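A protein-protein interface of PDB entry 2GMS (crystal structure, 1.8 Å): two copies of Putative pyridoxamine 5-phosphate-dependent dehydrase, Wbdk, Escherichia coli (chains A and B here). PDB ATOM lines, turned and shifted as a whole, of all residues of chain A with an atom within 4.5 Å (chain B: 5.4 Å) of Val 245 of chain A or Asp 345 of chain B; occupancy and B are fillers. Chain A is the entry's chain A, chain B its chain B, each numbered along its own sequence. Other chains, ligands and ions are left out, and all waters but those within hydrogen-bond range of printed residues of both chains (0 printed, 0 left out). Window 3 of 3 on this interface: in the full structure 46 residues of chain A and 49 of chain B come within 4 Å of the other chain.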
ATOM      1  N   CYS A 213      -2.228  16.072 -21.068  1.00  0.00           N
ATOM      2  CA  CYS A 213      -1.352  14.968 -20.737  1.00  0.00           C
ATOM      3  C   CYS A 213      -0.650  14.306 -21.935  1.00  0.00           C
ATOM      4  O   CYS A 213       0.584  14.133 -21.951  1.00  0.00           O
ATOM      5  CB  CYS A 213      -2.193  13.951 -19.928  1.00  0.00           C
ATOM      6  SG  CYS A 213      -1.335  12.431 -19.420  1.00  0.00           S
ATOM      7  N   GLY A 218       2.732  12.269 -21.860  1.00  0.00           N
ATOM      8  CA  GLY A 218       1.884  11.419 -21.024  1.00  0.00           C
ATOM      9  C   GLY A 218       2.172  11.630 -19.538  1.00  0.00           C
ATOM     10  O   GLY A 218       1.910  10.794 -18.682  1.00  0.00           O
ATOM     11  N   THR A 220       2.255  14.308 -15.936  1.00  0.00           N
ATOM     12  CA  THR A 220       1.324  15.094 -15.138  1.00  0.00           C
ATOM     13  C   THR A 220       1.706  16.561 -14.943  1.00  0.00           C
ATOM     14  O   THR A 220       0.964  17.343 -14.338  1.00  0.00           O
ATOM     15  CB  THR A 220       1.135  14.446 -13.736  1.00  0.00           C
ATOM     16  OG1 THR A 220       2.298  14.629 -12.964  1.00  0.00           O
ATOM     17  CG2 THR A 220       0.856  12.949 -13.807  1.00  0.00           C
ATOM     18  N   VAL A 229      -7.575  13.142 -14.734  1.00  0.00           N
ATOM     19  CA  VAL A 229      -6.824  11.968 -15.132  1.00  0.00           C
ATOM     20  C   VAL A 229      -6.276  11.242 -13.927  1.00  0.00           C
ATOM     21  O   VAL A 229      -6.413  10.043 -13.790  1.00  0.00           O
ATOM     22  CB  VAL A 229      -5.690  12.378 -16.055  1.00  0.00           C
ATOM     23  CG1 VAL A 229      -4.977  11.128 -16.521  1.00  0.00           C
ATOM     24  CG2 VAL A 229      -6.300  13.088 -17.266  1.00  0.00           C
ATOM     25  N   THR A 230      -5.643  11.987 -13.040  1.00  0.00           N
ATOM     26  CA  THR A 230      -5.078  11.349 -11.887  1.00  0.00           C
ATOM     27  C   THR A 230      -5.766  11.720 -10.600  1.00  0.00           C
ATOM     28  O   THR A 230      -5.359  11.241  -9.543  1.00  0.00           O
ATOM     29  CB  THR A 230      -3.563  11.569 -11.743  1.00  0.00           C
ATOM     30  OG1 THR A 230      -3.280  12.929 -11.420  1.00  0.00           O
ATOM     31  CG2 THR A 230      -2.881  11.152 -13.040  1.00  0.00           C
ATOM     32  N   LYS A 243       6.115  10.881 -13.485  1.00  0.00           N
ATOM     33  CA  LYS A 243       5.040   9.913 -13.558  1.00  0.00           C
ATOM     34  C   LYS A 243       4.273  10.038 -14.886  1.00  0.00           C
ATOM     35  O   LYS A 243       3.917  11.141 -15.313  1.00  0.00           O
ATOM     36  CB  LYS A 243       4.257   9.955 -12.251  1.00  0.00           C
ATOM     37  CG  LYS A 243       2.862  10.522 -12.282  1.00  0.00           C
ATOM     38  CD  LYS A 243       2.064  10.104 -11.050  1.00  0.00           C
ATOM     39  CE  LYS A 243       2.918  10.002  -9.784  1.00  0.00           C
ATOM     40  NZ  LYS A 243       2.222  10.464  -8.560  1.00  0.00           N
ATOM     41  N   PHE A 244       4.130   8.893 -15.577  1.00  0.00           N
ATOM     42  CA  PHE A 244       3.502   8.758 -16.883  1.00  0.00           C
ATOM     43  C   PHE A 244       2.238   7.960 -16.737  1.00  0.00           C
ATOM     44  O   PHE A 244       2.301   6.828 -16.261  1.00  0.00           O
ATOM     45  CB  PHE A 244       4.483   8.050 -17.820  1.00  0.00           C
ATOM     46  CG  PHE A 244       5.738   8.869 -17.874  1.00  0.00           C
ATOM     47  CD1 PHE A 244       6.877   8.521 -17.144  1.00  0.00           C
ATOM     48  CD2 PHE A 244       5.757  10.057 -18.602  1.00  0.00           C
ATOM     49  CE1 PHE A 244       8.015   9.328 -17.169  1.00  0.00           C
ATOM     50  CE2 PHE A 244       6.888  10.871 -18.648  1.00  0.00           C
ATOM     51  CZ  PHE A 244       8.021  10.504 -17.923  1.00  0.00           C
ATOM     52  N   VAL A 245       1.108   8.560 -17.123  1.00  0.00           N
ATOM     53  CA  VAL A 245      -0.187   7.921 -16.927  1.00  0.00           C
ATOM     54  C   VAL A 245      -0.983   7.529 -18.163  1.00  0.00           C
ATOM     55  O   VAL A 245      -1.938   6.741 -18.082  1.00  0.00           O
ATOM     56  CB  VAL A 245      -1.017   8.751 -15.928  1.00  0.00           C
ATOM     57  CG1 VAL A 245      -0.153   9.015 -14.705  1.00  0.00           C
ATOM     58  CG2 VAL A 245      -1.426  10.115 -16.496  1.00  0.00           C
ATOM     59  N   LEU A 246      -0.616   8.122 -19.289  1.00  0.00           N
ATOM     60  CA  LEU A 246      -1.299   7.858 -20.539  1.00  0.00           C
ATOM     61  C   LEU A 246      -0.290   7.801 -21.684  1.00  0.00           C
ATOM     62  O   LEU A 246       0.735   8.505 -21.719  1.00  0.00           O
ATOM     63  CB  LEU A 246      -2.428   8.870 -20.853  1.00  0.00           C
ATOM     64  CG  LEU A 246      -3.672   8.838 -19.956  1.00  0.00           C
ATOM     65  CD1 LEU A 246      -4.571  10.011 -20.338  1.00  0.00           C
ATOM     66  CD2 LEU A 246      -4.450   7.529 -20.144  1.00  0.00           C
ATOM     67  N   TYR B  95       5.992   4.360 -25.697  1.00  0.00           N
ATOM     68  CA  TYR B  95       4.678   4.589 -26.253  1.00  0.00           C
ATOM     69  C   TYR B  95       4.454   4.104 -27.699  1.00  0.00           C
ATOM     70  O   TYR B  95       3.443   3.494 -28.031  1.00  0.00           O
ATOM     71  CB  TYR B  95       4.275   6.057 -26.079  1.00  0.00           C
ATOM     72  CG  TYR B  95       4.175   6.568 -24.652  1.00  0.00           C
ATOM     73  CD1 TYR B  95       4.215   7.945 -24.437  1.00  0.00           C
ATOM     74  CD2 TYR B  95       3.968   5.735 -23.552  1.00  0.00           C
ATOM     75  CE1 TYR B  95       4.079   8.499 -23.168  1.00  0.00           C
ATOM     76  CE2 TYR B  95       3.829   6.274 -22.270  1.00  0.00           C
ATOM     77  CZ  TYR B  95       3.893   7.655 -22.077  1.00  0.00           C
ATOM     78  OH  TYR B  95       3.755   8.226 -20.836  1.00  0.00           O
ATOM     79  N   ASN B 343       4.910   2.561 -13.517  1.00  0.00           N
ATOM     80  CA  ASN B 343       3.768   3.283 -14.110  1.00  0.00           C
ATOM     81  C   ASN B 343       2.620   2.387 -14.547  1.00  0.00           C
ATOM     82  O   ASN B 343       2.328   2.250 -15.733  1.00  0.00           O
ATOM     83  CB  ASN B 343       4.274   4.169 -15.268  1.00  0.00           C
ATOM     84  CG  ASN B 343       5.344   5.124 -14.782  1.00  0.00           C
ATOM     85  OD1 ASN B 343       5.033   6.094 -14.069  1.00  0.00           O
ATOM     86  ND2 ASN B 343       6.600   4.855 -15.140  1.00  0.00           N
ATOM     87  N   THR B 344       1.975   1.789 -13.545  1.00  0.00           N
ATOM     88  CA  THR B 344       0.888   0.821 -13.686  1.00  0.00           C
ATOM     89  C   THR B 344      -0.330   1.238 -14.466  1.00  0.00           C
ATOM     90  O   THR B 344      -0.995   0.404 -15.078  1.00  0.00           O
ATOM     91  CB  THR B 344       0.512   0.190 -12.341  1.00  0.00           C
ATOM     92  OG1 THR B 344      -0.013   1.173 -11.465  1.00  0.00           O
ATOM     93  CG2 THR B 344       1.773  -0.425 -11.750  1.00  0.00           C
ATOM     94  N   ASP B 345      -0.592   2.531 -14.440  1.00  0.00           N
ATOM     95  CA  ASP B 345      -1.728   3.076 -15.124  1.00  0.00           C
ATOM     96  C   ASP B 345      -1.510   3.143 -16.609  1.00  0.00           C
ATOM     97  O   ASP B 345      -2.407   2.961 -17.417  1.00  0.00           O
ATOM     98  CB  ASP B 345      -2.001   4.459 -14.555  1.00  0.00           C
ATOM     99  CG  ASP B 345      -2.530   4.268 -13.166  1.00  0.00           C
ATOM    100  OD1 ASP B 345      -3.450   3.499 -12.922  1.00  0.00           O
ATOM    101  OD2 ASP B 345      -1.871   4.964 -12.266  1.00  0.00           O
ATOM    102  N   VAL B 346      -0.287   3.410 -16.983  1.00  0.00           N
ATOM    103  CA  VAL B 346      -0.109   3.488 -18.385  1.00  0.00           C
ATOM    104  C   VAL B 346       0.118   2.099 -18.957  1.00  0.00           C
ATOM    105  O   VAL B 346      -0.224   1.827 -20.107  1.00  0.00           O
ATOM    106  CB  VAL B 346       0.949   4.535 -18.731  1.00  0.00           C
ATOM    107  CG1 VAL B 346       2.356   4.033 -18.413  1.00  0.00           C
ATOM    108  CG2 VAL B 346       0.865   4.904 -20.205  1.00  0.00           C
ATOM    109  N   LEU B 347       0.683   1.206 -18.134  1.00  0.00           N
ATOM    110  CA  LEU B 347       1.005  -0.148 -18.574  1.00  0.00           C
ATOM    111  C   LEU B 347      -0.190  -1.003 -18.898  1.00  0.00           C
ATOM    112  O   LEU B 347      -0.069  -2.024 -19.568  1.00  0.00           O
ATOM    113  CB  LEU B 347       1.907  -0.870 -17.577  1.00  0.00           C
ATOM    114  CG  LEU B 347       3.331  -0.341 -17.646  1.00  0.00           C
ATOM    115  CD1 LEU B 347       4.082  -0.878 -16.444  1.00  0.00           C
ATOM    116  CD2 LEU B 347       4.005  -0.801 -18.938  1.00  0.00           C
ATOM    117  N   LYS B 348      -1.343  -0.569 -18.379  1.00  0.00           N
ATOM    118  CA  LYS B 348      -2.604  -1.249 -18.589  1.00  0.00           C
ATOM    119  C   LYS B 348      -2.912  -1.240 -20.066  1.00  0.00           C
ATOM    120  O   LYS B 348      -3.669  -2.075 -20.545  1.00  0.00           O
ATOM    121  CB  LYS B 348      -3.756  -0.572 -17.856  1.00  0.00           C
ATOM    122  CG  LYS B 348      -3.521  -0.463 -16.355  1.00  0.00           C
ATOM    123  CD  LYS B 348      -4.622   0.276 -15.617  1.00  0.00           C
ATOM    124  CE  LYS B 348      -5.375   1.257 -16.519  1.00  0.00           C
ATOM    125  NZ  LYS B 348      -5.090   2.679 -16.206  1.00  0.00           N
ATOM    126  N   TYR B 349      -2.322  -0.280 -20.784  1.00  0.00           N
ATOM    127  CA  TYR B 349      -2.558  -0.169 -22.209  1.00  0.00           C
ATOM    128  C   TYR B 349      -1.583  -1.003 -23.025  1.00  0.00           C
ATOM    129  O   TYR B 349      -1.774  -1.172 -24.239  1.00  0.00           O
ATOM    130  CB  TYR B 349      -2.527   1.291 -22.692  1.00  0.00           C
ATOM    131  CG  TYR B 349      -3.557   2.150 -21.998  1.00  0.00           C
ATOM    132  CD1 TYR B 349      -3.211   2.955 -20.912  1.00  0.00           C
ATOM    133  CD2 TYR B 349      -4.878   2.144 -22.440  1.00  0.00           C
ATOM    134  CE1 TYR B 349      -4.169   3.741 -20.275  1.00  0.00           C
ATOM    135  CE2 TYR B 349      -5.846   2.932 -21.821  1.00  0.00           C
ATOM    136  CZ  TYR B 349      -5.487   3.735 -20.740  1.00  0.00           C
ATOM    137  OH  TYR B 349      -6.434   4.517 -20.122  1.00  0.00           O
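The side-chain hydroxyl of Tyr 95 of chain B is in hydrogen-bond range of the backbone carbonyl oxygen of Leu 246 of chain A (3.2 Å). N of Phe 244 of chain A lies within hydrogen-bond range of OD1 of Asn 343 of chain B, 3.3 Å away.
The side-chain carboxylate of Asp 345 of chain B lies within salt-bridge range of the side-chain amino group of Lys 348 of chain B, at 3.8 Å. O of Gly 218 of chain A is in hydrogen-bond range of N of Val 245 of chain A (2.8 Å). N of Gly 218 of chain A lies within hydrogen-bond range of O of Cys 213 of chain A, at 2.8 Å.
Among the printed residues, merely in contact across the chains: Gly 218 of chain A with Tyr 95 of chain B (3.7 Å), Lys 243 of chain A with Asn 343 of chain B (3.9 Å), Phe 244 of chain A with Tyr 95 of chain B (3.1 Å), Phe 244 of chain A with Val 346 of chain B (3.5 Å), Val 245 of chain A with Asp 345 of chain B (3.9 Å), Val 245 of chain A with Val 346 of chain B (3.6 Å), Leu 246 of chain A with Val 346 of chain B (3.5 Å) and Leu 246 of chain A with Tyr 349 of chain B (3.6 Å).
Of the printed residues of chain B, Phe 244 of chain A touches Tyr 95, Asn 343 and Val 346. Val 245 of chain A touches two residues of chain B. Of the printed residues of chain B, Leu 246 of chain A touches Tyr 95 (3.2 Å), Val 346 (3.5 Å) and Tyr 349 (3.6 Å). Asp 345 of chain B touches just one residue of chain A: Val 245 (3.9 Å). Leu 347 of chain B touches none of the printed residues of chain A. Lys 348 of chain B touches none of the printed residues of chain A. The nearest residue of chain B that does not touch Val 245 of chain A is Tyr 349 of chain B (4.3 Å).
Hydrophobic or aromatic side chains of chain A that line the printed part of chain B: Phe 244 and Leu 246. Among the printed residues, 10 pairs touch across the chains. Among the printed residues, no Asp or Glu carboxylate lies within 4 Å of a Lys or Arg side-chain nitrogen of the other chain.
No position is printed for both chains.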
